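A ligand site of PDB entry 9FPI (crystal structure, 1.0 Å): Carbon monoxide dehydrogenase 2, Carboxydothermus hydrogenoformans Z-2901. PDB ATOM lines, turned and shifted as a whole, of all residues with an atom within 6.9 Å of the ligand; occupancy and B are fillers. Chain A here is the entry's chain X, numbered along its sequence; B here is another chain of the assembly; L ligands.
Gly 68 touches the ligand.
Ile 69 touches the ligand.
Met 199 touches the ligand (CG to S1, 3.5 Å).
Hydrophobic or aromatic side chains that line the ligand: Ile 69 and Met 199.
Of the 29 residues printed, 11 come within 4 Å of the ligand.
The backbone NH of Gln 53 lies close to the side-chain sulfur of Cys 51.
SD of Met 560 of chain B lies close to SG of Cys 51 (3.8 Å).
The backbone carbonyl oxygen (O) of Cys 56 is in hydrogen-bond range of the backbone NH (N) of Cys 48, 2.9 Å away.
The backbone NH (N) of Ile 69 lies close to the side-chain sulfur (SG) of Cys 56, at 3.5 Å.
NH2 of Arg 80 lies close to SG of Cys 48 (3.4 Å).
The backbone NH (N) of His 50 sits close to the side-chain sulfur (SG) of Cys 48.
The side-chain amide nitrogen (NE2) of Gln 38 of chain B sits at hydrogen-bond distance from the backbone carbonyl oxygen (O) of Gln 53 (2.9 Å).
A ring nitrogen (ND1) of His 50 is in hydrogen-bond range of the backbone carbonyl oxygen (O) of Thr 197.
N of Cys 51 sits close to S4 of the ligand.
The side-chain sulfur of Cys 51 binds an iron atom (FE2) of the ligand, at 2.3 Å.
The side-chain sulfur (SG) of Cys 56 binds an iron atom (FE1) of the ligand, at 2.3 Å.
The side-chain sulfur of Cys 48 binds an iron atom (FE3) of the ligand (2.3 Å).
S3 of the ligand sits close to N of Cys 70.
An iron atom (FE4) of the ligand is bound by the side-chain sulfur (SG) of Cys 70.
The backbone NH (N) of Gly 54 lies close to a sulfur (S4) of the ligand, at 3.7 Å.
S1 of the ligand sits close to NH2 of Arg 80, at 3.6 Å.
S3 of the ligand sits close to NE2 of Gln 53 (3.8 Å).
N of His 50 lies close to S4 of the ligand (3.8 Å).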
ATOM      1  N   CYS A  47     -21.202  -1.215 -21.538  1.00  0.00           N
ATOM      2  CA  CYS A  47     -21.914  -2.474 -21.356  1.00  0.00           C
ATOM      3  C   CYS A  47     -21.973  -3.181 -22.706  1.00  0.00           C
ATOM      4  O   CYS A  47     -22.157  -2.539 -23.745  1.00  0.00           O
ATOM      5  CB  CYS A  47     -23.340  -2.235 -20.848  1.00  0.00           C
ATOM      6  SG  CYS A  47     -24.271  -3.795 -20.662  1.00  0.00           S
ATOM      7  N   CYS A  48     -21.815  -4.490 -22.672  1.00  0.00           N
ATOM      8  CA  CYS A  48     -21.900  -5.337 -23.862  1.00  0.00           C
ATOM      9  C   CYS A  48     -22.692  -6.585 -23.554  1.00  0.00           C
ATOM     10  O   CYS A  48     -22.442  -7.274 -22.554  1.00  0.00           O
ATOM     11  CB  CYS A  48     -20.499  -5.735 -24.327  1.00  0.00           C
ATOM     12  SG  CYS A  48     -20.512  -6.730 -25.837  1.00  0.00           S
ATOM     13  N   ARG A  49     -23.638  -6.889 -24.447  1.00  0.00           N
ATOM     14  CA  ARG A  49     -24.453  -8.104 -24.404  1.00  0.00           C
ATOM     15  C   ARG A  49     -24.371  -8.838 -25.742  1.00  0.00           C
ATOM     16  O   ARG A  49     -25.339  -9.486 -26.165  1.00  0.00           O
ATOM     17  CB  ARG A  49     -25.894  -7.769 -24.029  1.00  0.00           C
ATOM     18  CG  ARG A  49     -26.021  -7.164 -22.652  1.00  0.00           C
ATOM     19  CD  ARG A  49     -27.393  -6.567 -22.446  1.00  0.00           C
ATOM     20  NE  ARG A  49     -28.415  -7.598 -22.574  1.00  0.00           N
ATOM     21  CZ  ARG A  49     -29.696  -7.371 -22.853  1.00  0.00           C
ATOM     22  NH1 ARG A  49     -30.168  -6.150 -22.985  1.00  0.00           N
ATOM     23  NH2 ARG A  49     -30.514  -8.412 -22.974  1.00  0.00           N
ATOM     24  N   HIS A  50     -23.235  -8.735 -26.424  1.00  0.00           N
ATOM     25  CA  HIS A  50     -23.095  -9.338 -27.752  1.00  0.00           C
ATOM     26  C   HIS A  50     -22.828 -10.849 -27.720  1.00  0.00           C
ATOM     27  O   HIS A  50     -22.759 -11.447 -28.791  1.00  0.00           O
ATOM     28  CB  HIS A  50     -22.055  -8.602 -28.588  1.00  0.00           C
ATOM     29  CG  HIS A  50     -22.454  -7.205 -28.940  1.00  0.00           C
ATOM     30  ND1 HIS A  50     -21.834  -6.500 -29.944  1.00  0.00           N
ATOM     31  CD2 HIS A  50     -23.377  -6.367 -28.414  1.00  0.00           C
ATOM     32  CE1 HIS A  50     -22.373  -5.285 -30.020  1.00  0.00           C
ATOM     33  NE2 HIS A  50     -23.303  -5.174 -29.097  1.00  0.00           N
ATOM     34  N   CYS A  51     -22.711 -11.474 -26.547  1.00  0.00           N
ATOM     35  CA  CYS A  51     -22.697 -12.939 -26.502  1.00  0.00           C
ATOM     36  C   CYS A  51     -23.248 -13.402 -25.170  1.00  0.00           C
ATOM     37  O   CYS A  51     -23.474 -12.605 -24.245  1.00  0.00           O
ATOM     38  CB  CYS A  51     -21.297 -13.519 -26.803  1.00  0.00           C
ATOM     39  SG  CYS A  51     -20.157 -13.538 -25.398  1.00  0.00           S
ATOM     40  N   LEU A  52     -23.410 -14.722 -25.041  1.00  0.00           N
ATOM     41  CA  LEU A  52     -24.021 -15.314 -23.859  1.00  0.00           C
ATOM     42  C   LEU A  52     -23.041 -15.514 -22.712  1.00  0.00           C
ATOM     43  O   LEU A  52     -23.436 -16.058 -21.674  1.00  0.00           O
ATOM     44  CB  LEU A  52     -24.713 -16.633 -24.206  1.00  0.00           C
ATOM     45  CG  LEU A  52     -25.782 -16.539 -25.293  1.00  0.00           C
ATOM     46  CD1 LEU A  52     -26.390 -17.918 -25.507  1.00  0.00           C
ATOM     47  CD2 LEU A  52     -26.848 -15.522 -24.931  1.00  0.00           C
ATOM     48  N   GLN A  53     -21.793 -15.078 -22.859  1.00  0.00           N
ATOM     49  CA  GLN A  53     -20.914 -14.935 -21.708  1.00  0.00           C
ATOM     50  C   GLN A  53     -21.223 -13.675 -20.936  1.00  0.00           C
ATOM     51  O   GLN A  53     -20.849 -13.565 -19.775  1.00  0.00           O
ATOM     52  CB  GLN A  53     -19.448 -14.964 -22.104  1.00  0.00           C
ATOM     53  CG  GLN A  53     -19.053 -16.336 -22.574  1.00  0.00           C
ATOM     54  CD  GLN A  53     -17.605 -16.503 -22.991  1.00  0.00           C
ATOM     55  OE1 GLN A  53     -17.086 -17.612 -22.999  1.00  0.00           O
ATOM     56  NE2 GLN A  53     -16.940 -15.420 -23.370  1.00  0.00           N
ATOM     57  N   GLY A  54     -21.902 -12.708 -21.566  1.00  0.00           N
ATOM     58  CA  GLY A  54     -22.276 -11.470 -20.909  1.00  0.00           C
ATOM     59  C   GLY A  54     -23.462 -11.669 -19.999  1.00  0.00           C
ATOM     60  O   GLY A  54     -23.944 -12.779 -19.771  1.00  0.00           O
ATOM     61  N   PRO A  55     -23.979 -10.576 -19.464  1.00  0.00           N
ATOM     62  CA  PRO A  55     -23.587  -9.197 -19.769  1.00  0.00           C
ATOM     63  C   PRO A  55     -22.229  -8.836 -19.187  1.00  0.00           C
ATOM     64  O   PRO A  55     -21.881  -9.205 -18.063  1.00  0.00           O
ATOM     65  CB  PRO A  55     -24.719  -8.391 -19.113  1.00  0.00           C
ATOM     66  CG  PRO A  55     -25.125  -9.239 -17.934  1.00  0.00           C
ATOM     67  CD  PRO A  55     -25.070 -10.637 -18.467  1.00  0.00           C
ATOM     68  N   CYS A  56     -21.459  -8.095 -19.974  1.00  0.00           N
ATOM     69  CA  CYS A  56     -20.217  -7.518 -19.531  1.00  0.00           C
ATOM     70  C   CYS A  56     -20.362  -6.014 -19.339  1.00  0.00           C
ATOM     71  O   CYS A  56     -21.147  -5.362 -20.022  1.00  0.00           O
ATOM     72  CB  CYS A  56     -19.114  -7.778 -20.569  1.00  0.00           C
ATOM     73  SG  CYS A  56     -18.624  -9.524 -20.644  1.00  0.00           S
ATOM     74  N   ARG A  57     -19.591  -5.485 -18.411  1.00  0.00           N
ATOM     75  CA  ARG A  57     -19.527  -4.052 -18.164  1.00  0.00           C
ATOM     76  C   ARG A  57     -18.100  -3.700 -17.797  1.00  0.00           C
ATOM     77  O   ARG A  57     -17.292  -4.560 -17.463  1.00  0.00           O
ATOM     78  CB  ARG A  57     -20.498  -3.669 -17.031  1.00  0.00           C
ATOM     79  CG  ARG A  57     -20.044  -4.156 -15.667  1.00  0.00           C
ATOM     80  CD  ARG A  57     -21.144  -4.165 -14.646  1.00  0.00           C
ATOM     81  NE  ARG A  57     -20.624  -4.548 -13.341  1.00  0.00           N
ATOM     82  CZ  ARG A  57     -20.201  -5.763 -13.035  1.00  0.00           C
ATOM     83  NH1 ARG A  57     -20.452  -6.803 -13.814  1.00  0.00           N
ATOM     84  NH2 ARG A  57     -19.520  -5.946 -11.909  1.00  0.00           N
ATOM     85  N   VAL A  67     -12.238  -4.750 -18.403  1.00  0.00           N
ATOM     86  CA  VAL A  67     -12.211  -5.287 -19.761  1.00  0.00           C
ATOM     87  C   VAL A  67     -13.308  -6.342 -19.840  1.00  0.00           C
ATOM     88  O   VAL A  67     -13.669  -6.953 -18.846  1.00  0.00           O
ATOM     89  CB  VAL A  67     -10.798  -5.838 -20.056  1.00  0.00           C
ATOM     90  CG1 VAL A  67     -10.432  -6.982 -19.108  1.00  0.00           C
ATOM     91  CG2 VAL A  67     -10.659  -6.238 -21.491  1.00  0.00           C
ATOM     92  N   GLY A  68     -13.857  -6.526 -21.040  1.00  0.00           N
ATOM     93  CA  GLY A  68     -14.860  -7.564 -21.229  1.00  0.00           C
ATOM     94  C   GLY A  68     -14.287  -8.951 -21.104  1.00  0.00           C
ATOM     95  O   GLY A  68     -13.083  -9.166 -21.174  1.00  0.00           O
ATOM     96  N   ILE A  69     -15.171  -9.929 -20.945  1.00  0.00           N
ATOM     97  CA  ILE A  69     -14.718 -11.298 -20.692  1.00  0.00           C
ATOM     98  C   ILE A  69     -13.863 -11.820 -21.839  1.00  0.00           C
ATOM     99  O   ILE A  69     -12.856 -12.497 -21.604  1.00  0.00           O
ATOM    100  CB  ILE A  69     -15.921 -12.212 -20.376  1.00  0.00           C
ATOM    101  CG1 ILE A  69     -16.465 -11.863 -18.977  1.00  0.00           C
ATOM    102  CG2 ILE A  69     -15.526 -13.675 -20.451  1.00  0.00           C
ATOM    103  CD1 ILE A  69     -17.797 -12.498 -18.647  1.00  0.00           C
ATOM    104  N   CYS A  70     -14.235 -11.549 -23.090  1.00  0.00           N
ATOM    105  CA  CYS A  70     -13.461 -11.982 -24.244  1.00  0.00           C
ATOM    106  C   CYS A  70     -12.198 -11.157 -24.471  1.00  0.00           C
ATOM    107  O   CYS A  70     -11.420 -11.465 -25.388  1.00  0.00           O
ATOM    108  CB  CYS A  70     -14.341 -11.897 -25.494  1.00  0.00           C
ATOM    109  SG  CYS A  70     -14.866 -10.192 -25.845  1.00  0.00           S
ATOM    110  N   GLY A  71     -11.977 -10.111 -23.670  1.00  0.00           N
ATOM    111  CA  GLY A  71     -10.884  -9.178 -23.889  1.00  0.00           C
ATOM    112  C   GLY A  71     -11.285  -7.873 -24.542  1.00  0.00           C
ATOM    113  O   GLY A  71     -10.413  -7.021 -24.765  1.00  0.00           O
ATOM    114  N   ALA A  72     -12.549  -7.682 -24.859  1.00  0.00           N
ATOM    115  CA  ALA A  72     -12.964  -6.436 -25.503  1.00  0.00           C
ATOM    116  C   ALA A  72     -12.723  -5.249 -24.591  1.00  0.00           C
ATOM    117  O   ALA A  72     -13.178  -5.209 -23.441  1.00  0.00           O
ATOM    118  CB  ALA A  72     -14.431  -6.531 -25.890  1.00  0.00           C
ATOM    119  N   THR A  73     -12.012  -4.253 -25.113  1.00  0.00           N
ATOM    120  CA  THR A  73     -11.706  -3.061 -24.337  1.00  0.00           C
ATOM    121  C   THR A  73     -12.889  -2.095 -24.344  1.00  0.00           C
ATOM    122  O   THR A  73     -13.861  -2.243 -25.094  1.00  0.00           O
ATOM    123  CB  THR A  73     -10.514  -2.333 -24.951  1.00  0.00           C
ATOM    124  OG1 THR A  73     -10.870  -1.950 -26.288  1.00  0.00           O
ATOM    125  CG2 THR A  73      -9.248  -3.182 -24.955  1.00  0.00           C
ATOM    126  N   ILE A  77     -15.923  -1.890 -27.061  1.00  0.00           N
ATOM    127  CA  ILE A  77     -17.321  -2.032 -26.648  1.00  0.00           C
ATOM    128  C   ILE A  77     -18.117  -0.791 -27.052  1.00  0.00           C
ATOM    129  O   ILE A  77     -19.208  -0.892 -27.627  1.00  0.00           O
ATOM    130  CB  ILE A  77     -17.378  -2.318 -25.142  1.00  0.00           C
ATOM    131  CG1 ILE A  77     -16.988  -3.780 -24.882  1.00  0.00           C
ATOM    132  CG2 ILE A  77     -18.762  -2.011 -24.575  1.00  0.00           C
ATOM    133  CD1 ILE A  77     -16.855  -4.132 -23.402  1.00  0.00           C
ATOM    134  N   ARG A  80     -18.522  -0.645 -30.912  1.00  0.00           N
ATOM    135  CA  ARG A  80     -19.444  -1.659 -31.423  1.00  0.00           C
ATOM    136  C   ARG A  80     -20.899  -1.278 -31.144  1.00  0.00           C
ATOM    137  O   ARG A  80     -21.763  -1.448 -32.009  1.00  0.00           O
ATOM    138  CB  ARG A  80     -19.136  -3.047 -30.854  1.00  0.00           C
ATOM    139  CG  ARG A  80     -17.792  -3.601 -31.285  1.00  0.00           C
ATOM    140  CD  ARG A  80     -17.624  -5.076 -30.947  1.00  0.00           C
ATOM    141  NE  ARG A  80     -17.804  -5.366 -29.523  1.00  0.00           N
ATOM    142  CZ  ARG A  80     -17.432  -6.508 -28.969  1.00  0.00           C
ATOM    143  NH1 ARG A  80     -16.820  -7.451 -29.682  1.00  0.00           N
ATOM    144  NH2 ARG A  80     -17.645  -6.718 -27.684  1.00  0.00           N
ATOM    145  N   THR A 197     -19.411  -6.361 -35.596  1.00  0.00           N
ATOM    146  CA  THR A 197     -19.609  -6.018 -34.190  1.00  0.00           C
ATOM    147  C   THR A 197     -20.011  -7.217 -33.341  1.00  0.00           C
ATOM    148  O   THR A 197     -20.118  -7.086 -32.117  1.00  0.00           O
ATOM    149  CB  THR A 197     -20.676  -4.921 -34.030  1.00  0.00           C
ATOM    150  OG1 THR A 197     -21.919  -5.370 -34.570  1.00  0.00           O
ATOM    151  CG2 THR A 197     -20.254  -3.608 -34.663  1.00  0.00           C
ATOM    152  N   SER A 198     -20.224  -8.378 -33.945  1.00  0.00           N
ATOM    153  CA  SER A 198     -20.494  -9.598 -33.204  1.00  0.00           C
ATOM    154  C   SER A 198     -19.206 -10.073 -32.529  1.00  0.00           C
ATOM    155  O   SER A 198     -18.110  -9.578 -32.793  1.00  0.00           O
ATOM    156  CB  SER A 198     -21.126 -10.656 -34.104  1.00  0.00           C
ATOM    157  OG  SER A 198     -20.216 -11.262 -35.003  1.00  0.00           O
ATOM    158  N   MET A 199     -19.359 -11.030 -31.618  1.00  0.00           N
ATOM    159  CA  MET A 199     -18.229 -11.398 -30.774  1.00  0.00           C
ATOM    160  C   MET A 199     -17.061 -11.940 -31.608  1.00  0.00           C
ATOM    161  O   MET A 199     -17.242 -12.718 -32.557  1.00  0.00           O
ATOM    162  CB  MET A 199     -18.673 -12.403 -29.714  1.00  0.00           C
ATOM    163  CG  MET A 199     -17.584 -12.797 -28.732  1.00  0.00           C
ATOM    164  SD  MET A 199     -16.584 -14.153 -29.389  1.00  0.00           S
ATOM    165  CE  MET A 199     -14.964 -13.795 -28.734  1.00  0.00           C
ATOM    166  N   GLY A 200     -15.867 -11.498 -31.246  1.00  0.00           N
ATOM    167  CA  GLY A 200     -14.670 -12.057 -31.828  1.00  0.00           C
ATOM    168  C   GLY A 200     -14.392 -11.643 -33.245  1.00  0.00           C
ATOM    169  O   GLY A 200     -13.679 -12.356 -33.974  1.00  0.00           O
ATOM    170  N   VAL B  28      -9.325 -15.586 -20.071  1.00  0.00           N
ATOM    171  CA  VAL B  28     -10.776 -15.458 -20.114  1.00  0.00           C
ATOM    172  C   VAL B  28     -11.432 -15.809 -18.788  1.00  0.00           C
ATOM    173  O   VAL B  28     -12.400 -15.168 -18.375  1.00  0.00           O
ATOM    174  CB  VAL B  28     -11.342 -16.281 -21.292  1.00  0.00           C
ATOM    175  CG1 VAL B  28     -11.109 -17.775 -21.108  1.00  0.00           C
ATOM    176  CG2 VAL B  28     -12.820 -15.981 -21.516  1.00  0.00           C
ATOM    177  N   MET B  35     -15.673 -10.064 -13.543  1.00  0.00           N
ATOM    178  CA  MET B  35     -16.974  -9.552 -13.958  1.00  0.00           C
ATOM    179  C   MET B  35     -18.094  -9.902 -12.983  1.00  0.00           C
ATOM    180  O   MET B  35     -19.185  -9.322 -13.089  1.00  0.00           O
ATOM    181  CB  MET B  35     -17.321 -10.090 -15.371  1.00  0.00           C
ATOM    182  CG  MET B  35     -18.428  -9.278 -16.000  1.00  0.00           C
ATOM    183  SD  MET B  35     -17.910  -7.604 -16.464  1.00  0.00           S
ATOM    184  CE  MET B  35     -16.526  -7.894 -17.548  1.00  0.00           C
ATOM    185  N   GLN B  38     -22.476 -10.559 -12.339  1.00  0.00           N
ATOM    186  CA  GLN B  38     -22.933  -9.936 -13.557  1.00  0.00           C
ATOM    187  C   GLN B  38     -24.309  -9.296 -13.367  1.00  0.00           C
ATOM    188  O   GLN B  38     -25.075  -9.634 -12.460  1.00  0.00           O
ATOM    189  CB  GLN B  38     -22.936 -10.944 -14.702  1.00  0.00           C
ATOM    190  CG  GLN B  38     -21.526 -11.376 -15.083  1.00  0.00           C
ATOM    191  CD  GLN B  38     -21.506 -12.436 -16.142  1.00  0.00           C
ATOM    192  OE1 GLN B  38     -21.689 -13.613 -15.867  1.00  0.00           O
ATOM    193  NE2 GLN B  38     -21.267 -12.019 -17.374  1.00  0.00           N
ATOM    194  N   PRO B 336     -10.331 -11.003 -28.507  1.00  0.00           N
ATOM    195  CA  PRO B 336      -9.328  -9.972 -28.843  1.00  0.00           C
ATOM    196  C   PRO B 336      -8.184  -9.916 -27.852  1.00  0.00           C
ATOM    197  O   PRO B 336      -7.146  -9.304 -28.167  1.00  0.00           O
ATOM    198  CB  PRO B 336     -10.149  -8.679 -28.918  1.00  0.00           C
ATOM    199  CG  PRO B 336     -11.360  -8.956 -28.087  1.00  0.00           C
ATOM    200  CD  PRO B 336     -11.676 -10.418 -28.302  1.00  0.00           C
ATOM    201  N   MET B 560     -22.497 -19.774 -26.797  1.00  0.00           N
ATOM    202  CA  MET B 560     -21.926 -18.458 -26.521  1.00  0.00           C
ATOM    203  C   MET B 560     -22.297 -17.419 -27.587  1.00  0.00           C
ATOM    204  O   MET B 560     -22.856 -16.364 -27.267  1.00  0.00           O
ATOM    205  CB  MET B 560     -20.394 -18.580 -26.354  1.00  0.00           C
ATOM    206  CG  MET B 560     -19.612 -17.276 -26.133  1.00  0.00           C
ATOM    207  SD  MET B 560     -19.070 -16.406 -27.627  1.00  0.00           S
ATOM    208  CE  MET B 560     -17.971 -17.609 -28.372  1.00  0.00           C
HETATM  209 FE1  LIG L   1     -18.661  -9.894 -22.929  1.00  0.00          FE
HETATM  210 FE2  LIG L   1     -19.479 -11.382 -25.025  1.00  0.00          FE
HETATM  211 FE3  LIG L   1     -19.456  -8.682 -25.169  1.00  0.00          FE
HETATM  212 FE4  LIG L   1     -17.084  -9.998 -25.153  1.00  0.00          FE
HETATM  213  S1  LIG L   1     -18.734 -10.061 -26.804  1.00  0.00           S
HETATM  214  S2  LIG L   1     -17.560  -8.138 -23.981  1.00  0.00           S
HETATM  215  S3  LIG L   1     -17.606 -11.744 -23.700  1.00  0.00           S
HETATM  216  S4  LIG L   1     -20.799  -9.980 -23.844  1.00  0.00           S
